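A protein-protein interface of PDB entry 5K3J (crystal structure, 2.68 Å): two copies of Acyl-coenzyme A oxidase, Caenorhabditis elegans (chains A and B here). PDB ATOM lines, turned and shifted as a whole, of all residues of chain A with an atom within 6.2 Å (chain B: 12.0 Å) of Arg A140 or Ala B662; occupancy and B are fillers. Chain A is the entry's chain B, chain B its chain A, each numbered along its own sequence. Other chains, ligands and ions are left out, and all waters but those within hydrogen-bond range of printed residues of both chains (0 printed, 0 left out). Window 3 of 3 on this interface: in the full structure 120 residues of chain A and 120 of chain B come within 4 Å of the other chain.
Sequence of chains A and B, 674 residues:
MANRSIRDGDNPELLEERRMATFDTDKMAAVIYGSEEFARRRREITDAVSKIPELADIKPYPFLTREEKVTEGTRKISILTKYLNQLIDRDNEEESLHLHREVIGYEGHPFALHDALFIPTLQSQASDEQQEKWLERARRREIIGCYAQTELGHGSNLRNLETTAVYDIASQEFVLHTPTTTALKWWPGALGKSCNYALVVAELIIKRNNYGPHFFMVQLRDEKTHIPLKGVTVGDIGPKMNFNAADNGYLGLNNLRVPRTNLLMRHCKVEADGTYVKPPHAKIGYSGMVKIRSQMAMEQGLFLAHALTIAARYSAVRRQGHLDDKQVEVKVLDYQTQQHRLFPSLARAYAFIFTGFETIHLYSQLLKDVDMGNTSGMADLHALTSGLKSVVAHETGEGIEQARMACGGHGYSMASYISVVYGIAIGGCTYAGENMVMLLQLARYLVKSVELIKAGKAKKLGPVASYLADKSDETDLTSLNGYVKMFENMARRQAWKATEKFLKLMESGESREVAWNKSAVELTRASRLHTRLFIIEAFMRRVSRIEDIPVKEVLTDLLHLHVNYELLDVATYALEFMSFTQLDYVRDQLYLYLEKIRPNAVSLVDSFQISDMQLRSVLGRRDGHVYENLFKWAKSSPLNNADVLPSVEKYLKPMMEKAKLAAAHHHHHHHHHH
Along chain A the printed residues that touch a printed residue of chain B span positions 137 to 143.
Of the 14 printed residues of chain B, 4 touch a printed residue of chain A.
Hydrophobic or aromatic side chains of chain B within 4 Å of the printed part of chain A: Met B656 and Ala B659.
Among the printed residues, 8 pairs touch across the chains.
Among the printed residues, pairs that only touch across the chains: Arg A137 with Lys B660 (3.9 Å), Arg A140 with Ala B662 (3.5 Å), Arg A141 with Ala B659 (3.5 Å), Glu A142 with Met B656 (3.6 Å), Glu A142 with Ala B659 (3.6 Å), Glu A142 with Lys B660 (3.3 Å) and Ile A143 with Met B656 (3.6 Å).
The guanidinium group (NH1) of Arg A141 lies within hydrogen-bond range of the side-chain hydroxyl (OG1) of Thr A81.
The side-chain carboxylate of Glu A142 is in salt-bridge range of the guanidinium group of Arg A140, 3.8 Å away.
NE of Arg A137 is in salt-bridge range of OE1 of Glu A142 (2.7 Å).
Arg A140 touches just these residues of chain B: Ala B659 and Ala B662.
Of the printed residues of chain A, Ala B662 touches Arg A140 (3.5 Å).
No residue of chain B comes within 4 Å of Glu A136.
No residue of chain B comes within 4 Å of Ala A138.
Of the printed residues of chain A, Ala B659 touches Arg A140, Arg A141 and Glu A142.
Printed residues of chain B within 4 Å of Arg A141: Ala B659 (3.5 Å).
Leu B652 touches none of the printed residues of chain A.
His A114 touches none of the printed residues of chain B.
The nearest residue of chain B that does not touch Arg A140 is Ala B663 (4.05 Å).
The nearest residue of chain A that does not touch Ala B662 is Glu A142 (5.8 Å).
The nearest printed residue of chain A that does not touch Lys B660 is Arg A140 (4.6 Å).
NH1 of Arg A140 sits at hydrogen-bond distance from O of Ala B659 (3.5 Å).
No position is printed for both chains.
Of the 8 pairs that touch across the chains among the printed residues, none has its exchanged pair printed and touching as well.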
ATOM      1  N   THR A  81      -7.096 -10.448  27.506  1.00  0.00           N
ATOM      2  CA  THR A  81      -7.629 -10.723  26.177  1.00  0.00           C
ATOM      3  C   THR A  81      -8.848  -9.860  25.848  1.00  0.00           C
ATOM      4  O   THR A  81      -9.035  -9.458  24.701  1.00  0.00           O
ATOM      5  CB  THR A  81      -8.005 -12.216  26.038  1.00  0.00           C
ATOM      6  OG1 THR A  81      -6.860 -13.026  26.336  1.00  0.00           O
ATOM      7  CG2 THR A  81      -8.484 -12.534  24.627  1.00  0.00           C
ATOM      8  N   ARG A  90      -2.836  -5.982  18.279  1.00  0.00           N
ATOM      9  CA  ARG A  90      -2.769  -7.428  18.524  1.00  0.00           C
ATOM     10  C   ARG A  90      -1.657  -8.180  17.789  1.00  0.00           C
ATOM     11  O   ARG A  90      -1.053  -9.105  18.335  1.00  0.00           O
ATOM     12  CB  ARG A  90      -4.110  -8.067  18.158  1.00  0.00           C
ATOM     13  CG  ARG A  90      -4.204  -9.553  18.487  1.00  0.00           C
ATOM     14  CD  ARG A  90      -5.241 -10.258  17.600  1.00  0.00           C
ATOM     15  NE  ARG A  90      -4.729 -10.517  16.256  1.00  0.00           N
ATOM     16  CZ  ARG A  90      -5.458 -11.055  15.282  1.00  0.00           C
ATOM     17  NH1 ARG A  90      -6.730 -11.383  15.505  1.00  0.00           N
ATOM     18  NH2 ARG A  90      -4.924 -11.265  14.082  1.00  0.00           N
ATOM     19  N   HIS A 114       1.329 -20.957  23.000  1.00  0.00           N
ATOM     20  CA  HIS A 114       0.404 -20.684  21.907  1.00  0.00           C
ATOM     21  C   HIS A 114       0.960 -19.577  21.023  1.00  0.00           C
ATOM     22  O   HIS A 114       0.939 -19.663  19.792  1.00  0.00           O
ATOM     23  CB  HIS A 114      -0.970 -20.291  22.456  1.00  0.00           C
ATOM     24  CG  HIS A 114      -1.942 -19.848  21.408  1.00  0.00           C
ATOM     25  ND1 HIS A 114      -2.765 -20.729  20.735  1.00  0.00           N
ATOM     26  CD2 HIS A 114      -2.231 -18.621  20.917  1.00  0.00           C
ATOM     27  CE1 HIS A 114      -3.514 -20.062  19.877  1.00  0.00           C
ATOM     28  NE2 HIS A 114      -3.210 -18.779  19.965  1.00  0.00           N
ATOM     29  N   LEU A 135      -4.853 -20.473  11.588  1.00  0.00           N
ATOM     30  CA  LEU A 135      -3.945 -19.411  12.039  1.00  0.00           C
ATOM     31  C   LEU A 135      -4.650 -18.185  12.624  1.00  0.00           C
ATOM     32  O   LEU A 135      -4.180 -17.606  13.606  1.00  0.00           O
ATOM     33  CB  LEU A 135      -3.033 -18.965  10.894  1.00  0.00           C
ATOM     34  CG  LEU A 135      -1.996 -17.903  11.273  1.00  0.00           C
ATOM     35  CD1 LEU A 135      -1.150 -18.382  12.451  1.00  0.00           C
ATOM     36  CD2 LEU A 135      -1.125 -17.557  10.076  1.00  0.00           C
ATOM     37  N   GLU A 136      -5.780 -17.805  12.039  1.00  0.00           N
ATOM     38  CA  GLU A 136      -6.546 -16.675  12.547  1.00  0.00           C
ATOM     39  C   GLU A 136      -7.428 -17.087  13.724  1.00  0.00           C
ATOM     40  O   GLU A 136      -7.770 -16.263  14.568  1.00  0.00           O
ATOM     41  CB  GLU A 136      -7.393 -16.044  11.443  1.00  0.00           C
ATOM     42  CG  GLU A 136      -8.161 -14.810  11.889  1.00  0.00           C
ATOM     43  CD  GLU A 136      -7.259 -13.619  12.153  1.00  0.00           C
ATOM     44  OE1 GLU A 136      -6.039 -13.728  11.915  1.00  0.00           O
ATOM     45  OE2 GLU A 136      -7.772 -12.574  12.599  1.00  0.00           O
ATOM     46  N   ARG A 137      -7.791 -18.364  13.773  1.00  0.00           N
ATOM     47  CA  ARG A 137      -8.543 -18.901  14.899  1.00  0.00           C
ATOM     48  C   ARG A 137      -7.637 -18.891  16.118  1.00  0.00           C
ATOM     49  O   ARG A 137      -8.084 -18.718  17.250  1.00  0.00           O
ATOM     50  CB  ARG A 137      -8.997 -20.329  14.602  1.00  0.00           C
ATOM     51  CG  ARG A 137     -10.266 -20.421  13.778  1.00  0.00           C
ATOM     52  CD  ARG A 137     -10.970 -21.743  14.009  1.00  0.00           C
ATOM     53  NE  ARG A 137     -11.874 -21.685  15.152  1.00  0.00           N
ATOM     54  CZ  ARG A 137     -12.346 -22.752  15.786  1.00  0.00           C
ATOM     55  NH1 ARG A 137     -12.000 -23.969  15.388  1.00  0.00           N
ATOM     56  NH2 ARG A 137     -13.164 -22.605  16.819  1.00  0.00           N
ATOM     57  N   ALA A 138      -6.350 -19.080  15.860  1.00  0.00           N
ATOM     58  CA  ALA A 138      -5.310 -19.023  16.877  1.00  0.00           C
ATOM     59  C   ALA A 138      -5.145 -17.605  17.413  1.00  0.00           C
ATOM     60  O   ALA A 138      -5.191 -17.377  18.623  1.00  0.00           O
ATOM     61  CB  ALA A 138      -4.001 -19.528  16.309  1.00  0.00           C
ATOM     62  N   ARG A 139      -4.955 -16.658  16.498  1.00  0.00           N
ATOM     63  CA  ARG A 139      -4.741 -15.255  16.845  1.00  0.00           C
ATOM     64  C   ARG A 139      -5.961 -14.638  17.518  1.00  0.00           C
ATOM     65  O   ARG A 139      -5.839 -13.707  18.319  1.00  0.00           O
ATOM     66  CB  ARG A 139      -4.376 -14.457  15.596  1.00  0.00           C
ATOM     67  CG  ARG A 139      -2.930 -14.638  15.154  1.00  0.00           C
ATOM     68  CD  ARG A 139      -2.726 -14.237  13.693  1.00  0.00           C
ATOM     69  NE  ARG A 139      -1.423 -13.612  13.491  1.00  0.00           N
ATOM     70  CZ  ARG A 139      -0.869 -13.385  12.301  1.00  0.00           C
ATOM     71  NH1 ARG A 139      -1.497 -13.743  11.183  1.00  0.00           N
ATOM     72  NH2 ARG A 139       0.322 -12.803  12.227  1.00  0.00           N
ATOM     73  N   ARG A 140      -7.139 -15.160  17.192  1.00  0.00           N
ATOM     74  CA  ARG A 140      -8.377 -14.701  17.811  1.00  0.00           C
ATOM     75  C   ARG A 140      -8.573 -15.408  19.147  1.00  0.00           C
ATOM     76  O   ARG A 140      -9.554 -15.176  19.852  1.00  0.00           O
ATOM     77  CB  ARG A 140      -9.569 -14.968  16.892  1.00  0.00           C
ATOM     78  CG  ARG A 140      -9.835 -13.863  15.883  1.00  0.00           C
ATOM     79  CD  ARG A 140      -9.857 -14.403  14.464  1.00  0.00           C
ATOM     80  NE  ARG A 140     -11.176 -14.274  13.850  1.00  0.00           N
ATOM     81  CZ  ARG A 140     -12.241 -13.774  14.468  1.00  0.00           C
ATOM     82  NH1 ARG A 140     -12.147 -13.354  15.721  1.00  0.00           N
ATOM     83  NH2 ARG A 140     -13.402 -13.694  13.831  1.00  0.00           N
ATOM     84  N   ARG A 141      -7.622 -16.275  19.482  1.00  0.00           N
ATOM     85  CA  ARG A 141      -7.656 -17.034  20.728  1.00  0.00           C
ATOM     86  C   ARG A 141      -9.006 -17.725  20.876  1.00  0.00           C
ATOM     87  O   ARG A 141      -9.591 -17.765  21.961  1.00  0.00           O
ATOM     88  CB  ARG A 141      -7.342 -16.131  21.922  1.00  0.00           C
ATOM     89  CG  ARG A 141      -5.910 -15.629  21.885  1.00  0.00           C
ATOM     90  CD  ARG A 141      -5.570 -14.819  23.118  1.00  0.00           C
ATOM     91  NE  ARG A 141      -4.138 -14.569  23.215  1.00  0.00           N
ATOM     92  CZ  ARG A 141      -3.586 -13.759  24.114  1.00  0.00           C
ATOM     93  NH1 ARG A 141      -4.347 -13.106  24.991  1.00  0.00           N
ATOM     94  NH2 ARG A 141      -2.270 -13.593  24.133  1.00  0.00           N
ATOM     95  N   GLU A 142      -9.493 -18.251  19.751  1.00  0.00           N
ATOM     96  CA  GLU A 142     -10.664 -19.118  19.728  1.00  0.00           C
ATOM     97  C   GLU A 142     -10.244 -20.494  20.209  1.00  0.00           C
ATOM     98  O   GLU A 142     -11.045 -21.243  20.771  1.00  0.00           O
ATOM     99  CB  GLU A 142     -11.268 -19.215  18.323  1.00  0.00           C
ATOM    100  CG  GLU A 142     -11.743 -17.896  17.747  1.00  0.00           C
ATOM    101  CD  GLU A 142     -12.507 -18.064  16.448  1.00  0.00           C
ATOM    102  OE1 GLU A 142     -12.649 -19.214  15.984  1.00  0.00           O
ATOM    103  OE2 GLU A 142     -12.972 -17.043  15.895  1.00  0.00           O
ATOM    104  N   ILE A 143      -8.977 -20.822  19.973  1.00  0.00           N
ATOM    105  CA  ILE A 143      -8.412 -22.096  20.398  1.00  0.00           C
ATOM    106  C   ILE A 143      -7.043 -21.903  21.046  1.00  0.00           C
ATOM    107  O   ILE A 143      -6.341 -20.936  20.761  1.00  0.00           O
ATOM    108  CB  ILE A 143      -8.275 -23.075  19.211  1.00  0.00           C
ATOM    109  CG1 ILE A 143      -7.340 -22.489  18.142  1.00  0.00           C
ATOM    110  CG2 ILE A 143      -9.646 -23.402  18.629  1.00  0.00           C
ATOM    111  CD1 ILE A 143      -7.147 -23.387  16.950  1.00  0.00           C
ATOM    112  N   TYR B 651     -12.794 -19.508  33.438  1.00  0.00           N
ATOM    113  CA  TYR B 651     -12.191 -18.423  32.664  1.00  0.00           C
ATOM    114  C   TYR B 651     -11.943 -18.745  31.191  1.00  0.00           C
ATOM    115  O   TYR B 651     -12.270 -17.945  30.317  1.00  0.00           O
ATOM    116  CB  TYR B 651     -10.859 -17.983  33.289  1.00  0.00           C
ATOM    117  CG  TYR B 651     -10.963 -17.345  34.656  1.00  0.00           C
ATOM    118  CD1 TYR B 651     -11.522 -16.084  34.814  1.00  0.00           C
ATOM    119  CD2 TYR B 651     -10.479 -17.993  35.787  1.00  0.00           C
ATOM    120  CE1 TYR B 651     -11.614 -15.492  36.060  1.00  0.00           C
ATOM    121  CE2 TYR B 651     -10.568 -17.411  37.040  1.00  0.00           C
ATOM    122  CZ  TYR B 651     -11.137 -16.156  37.171  1.00  0.00           C
ATOM    123  OH  TYR B 651     -11.228 -15.564  38.409  1.00  0.00           O
ATOM    124  N   LEU B 652     -11.340 -19.897  30.917  1.00  0.00           N
ATOM    125  CA  LEU B 652     -10.894 -20.203  29.560  1.00  0.00           C
ATOM    126  C   LEU B 652     -12.041 -20.553  28.619  1.00  0.00           C
ATOM    127  O   LEU B 652     -11.998 -20.212  27.436  1.00  0.00           O
ATOM    128  CB  LEU B 652      -9.875 -21.344  29.573  1.00  0.00           C
ATOM    129  CG  LEU B 652      -8.466 -20.961  30.029  1.00  0.00           C
ATOM    130  CD1 LEU B 652      -7.469 -22.058  29.682  1.00  0.00           C
ATOM    131  CD2 LEU B 652      -8.038 -19.627  29.432  1.00  0.00           C
ATOM    132  N   LYS B 653     -13.057 -21.238  29.136  1.00  0.00           N
ATOM    133  CA  LYS B 653     -14.217 -21.595  28.325  1.00  0.00           C
ATOM    134  C   LYS B 653     -15.012 -20.348  27.901  1.00  0.00           C
ATOM    135  O   LYS B 653     -15.272 -20.171  26.712  1.00  0.00           O
ATOM    136  CB  LYS B 653     -15.115 -22.596  29.073  1.00  0.00           C
ATOM    137  CG  LYS B 653     -14.456 -23.947  29.334  1.00  0.00           C
ATOM    138  CD  LYS B 653     -15.099 -25.050  28.509  1.00  0.00           C
ATOM    139  CE  LYS B 653     -16.350 -25.594  29.184  1.00  0.00           C
ATOM    140  NZ  LYS B 653     -16.033 -26.642  30.196  1.00  0.00           N
ATOM    141  N   PRO B 654     -15.382 -19.468  28.855  1.00  0.00           N
ATOM    142  CA  PRO B 654     -16.120 -18.273  28.425  1.00  0.00           C
ATOM    143  C   PRO B 654     -15.295 -17.343  27.537  1.00  0.00           C
ATOM    144  O   PRO B 654     -15.844 -16.700  26.642  1.00  0.00           O
ATOM    145  CB  PRO B 654     -16.469 -17.579  29.751  1.00  0.00           C
ATOM    146  CG  PRO B 654     -16.378 -18.635  30.776  1.00  0.00           C
ATOM    147  CD  PRO B 654     -15.258 -19.510  30.324  1.00  0.00           C
ATOM    148  N   MET B 655     -13.993 -17.274  27.790  1.00  0.00           N
ATOM    149  CA  MET B 655     -13.094 -16.477  26.967  1.00  0.00           C
ATOM    150  C   MET B 655     -13.123 -16.950  25.517  1.00  0.00           C
ATOM    151  O   MET B 655     -13.218 -16.140  24.593  1.00  0.00           O
ATOM    152  CB  MET B 655     -11.670 -16.549  27.513  1.00  0.00           C
ATOM    153  CG  MET B 655     -10.651 -15.817  26.668  1.00  0.00           C
ATOM    154  SD  MET B 655      -9.013 -16.538  26.841  1.00  0.00           S
ATOM    155  CE  MET B 655      -9.368 -18.213  26.320  1.00  0.00           C
ATOM    156  N   MET B 656     -13.051 -18.266  25.330  1.00  0.00           N
ATOM    157  CA  MET B 656     -12.990 -18.862  23.998  1.00  0.00           C
ATOM    158  C   MET B 656     -14.284 -18.664  23.219  1.00  0.00           C
ATOM    159  O   MET B 656     -14.247 -18.326  22.039  1.00  0.00           O
ATOM    160  CB  MET B 656     -12.667 -20.354  24.095  1.00  0.00           C
ATOM    161  CG  MET B 656     -11.198 -20.663  24.304  1.00  0.00           C
ATOM    162  SD  MET B 656     -10.955 -22.396  24.722  1.00  0.00           S
ATOM    163  CE  MET B 656      -9.513 -22.794  23.747  1.00  0.00           C
ATOM    164  N   GLU B 657     -15.417 -18.880  23.881  1.00  0.00           N
ATOM    165  CA  GLU B 657     -16.724 -18.641  23.278  1.00  0.00           C
ATOM    166  C   GLU B 657     -16.815 -17.225  22.736  1.00  0.00           C
ATOM    167  O   GLU B 657     -17.223 -17.005  21.595  1.00  0.00           O
ATOM    168  CB  GLU B 657     -17.837 -18.875  24.299  1.00  0.00           C
ATOM    169  CG  GLU B 657     -19.209 -18.450  23.823  1.00  0.00           C
ATOM    170  CD  GLU B 657     -19.694 -19.264  22.638  1.00  0.00           C
ATOM    171  OE1 GLU B 657     -19.246 -20.421  22.474  1.00  0.00           O
ATOM    172  OE2 GLU B 657     -20.521 -18.737  21.864  1.00  0.00           O
ATOM    173  N   LYS B 658     -16.418 -16.273  23.571  1.00  0.00           N
ATOM    174  CA  LYS B 658     -16.476 -14.861  23.225  1.00  0.00           C
ATOM    175  C   LYS B 658     -15.614 -14.536  22.009  1.00  0.00           C
ATOM    176  O   LYS B 658     -16.031 -13.780  21.131  1.00  0.00           O
ATOM    177  CB  LYS B 658     -16.037 -14.010  24.416  1.00  0.00           C
ATOM    178  CG  LYS B 658     -16.057 -12.522  24.139  1.00  0.00           C
ATOM    179  CD  LYS B 658     -16.018 -11.725  25.428  1.00  0.00           C
ATOM    180  CE  LYS B 658     -16.356 -10.264  25.183  1.00  0.00           C
ATOM    181  NZ  LYS B 658     -16.318  -9.467  26.440  1.00  0.00           N
ATOM    182  N   ALA B 659     -14.422 -15.120  21.957  1.00  0.00           N
ATOM    183  CA  ALA B 659     -13.466 -14.835  20.894  1.00  0.00           C
ATOM    184  C   ALA B 659     -13.983 -15.291  19.533  1.00  0.00           C
ATOM    185  O   ALA B 659     -13.715 -14.657  18.513  1.00  0.00           O
ATOM    186  CB  ALA B 659     -12.137 -15.491  21.199  1.00  0.00           C
ATOM    187  N   LYS B 660     -14.728 -16.389  19.523  1.00  0.00           N
ATOM    188  CA  LYS B 660     -15.247 -16.937  18.277  1.00  0.00           C
ATOM    189  C   LYS B 660     -16.324 -16.045  17.686  1.00  0.00           C
ATOM    190  O   LYS B 660     -16.421 -15.895  16.467  1.00  0.00           O
ATOM    191  CB  LYS B 660     -15.806 -18.336  18.503  1.00  0.00           C
ATOM    192  CG  LYS B 660     -14.805 -19.263  19.154  1.00  0.00           C
ATOM    193  CD  LYS B 660     -15.450 -20.478  19.779  1.00  0.00           C
ATOM    194  CE  LYS B 660     -14.371 -21.366  20.369  1.00  0.00           C
ATOM    195  NZ  LYS B 660     -14.932 -22.491  21.158  1.00  0.00           N
ATOM    196  N   LEU B 661     -17.139 -15.456  18.552  1.00  0.00           N
ATOM    197  CA  LEU B 661     -18.244 -14.625  18.097  1.00  0.00           C
ATOM    198  C   LEU B 661     -17.804 -13.204  17.753  1.00  0.00           C
ATOM    199  O   LEU B 661     -18.470 -12.520  16.978  1.00  0.00           O
ATOM    200  CB  LEU B 661     -19.339 -14.587  19.164  1.00  0.00           C
ATOM    201  CG  LEU B 661     -19.855 -15.938  19.674  1.00  0.00           C
ATOM    202  CD1 LEU B 661     -20.922 -15.742  20.748  1.00  0.00           C
ATOM    203  CD2 LEU B 661     -20.383 -16.810  18.537  1.00  0.00           C
ATOM    204  N   ALA B 662     -16.685 -12.772  18.335  1.00  0.00           N
ATOM    205  CA  ALA B 662     -16.209 -11.392  18.210  1.00  0.00           C
ATOM    206  C   ALA B 662     -15.888 -11.011  16.772  1.00  0.00           C
ATOM    207  O   ALA B 662     -15.537 -11.860  15.953  1.00  0.00           O
ATOM    208  CB  ALA B 662     -14.984 -11.168  19.090  1.00  0.00           C
ATOM    209  N   ALA B 663     -16.005  -9.719  16.482  1.00  0.00           N
ATOM    210  CA  ALA B 663     -15.848  -9.205  15.129  1.00  0.00           C
ATOM    211  C   ALA B 663     -14.429  -9.378  14.594  1.00  0.00           C
ATOM    212  O   ALA B 663     -13.482  -9.552  15.360  1.00  0.00           O
ATOM    213  CB  ALA B 663     -16.252  -7.741  15.083  1.00  0.00           C
ATOM    214  N   ALA B 664     -14.298  -9.331  13.271  1.00  0.00           N
ATOM    215  CA  ALA B 664     -13.007  -9.492  12.608  1.00  0.00           C
ATOM    216  C   ALA B 664     -12.204  -8.196  12.652  1.00  0.00           C
ATOM    217  O   ALA B 664     -11.676  -7.815  13.695  1.00  0.00           O
ATOM    218  CB  ALA B 664     -13.204  -9.943  11.169  1.00  0.00           C
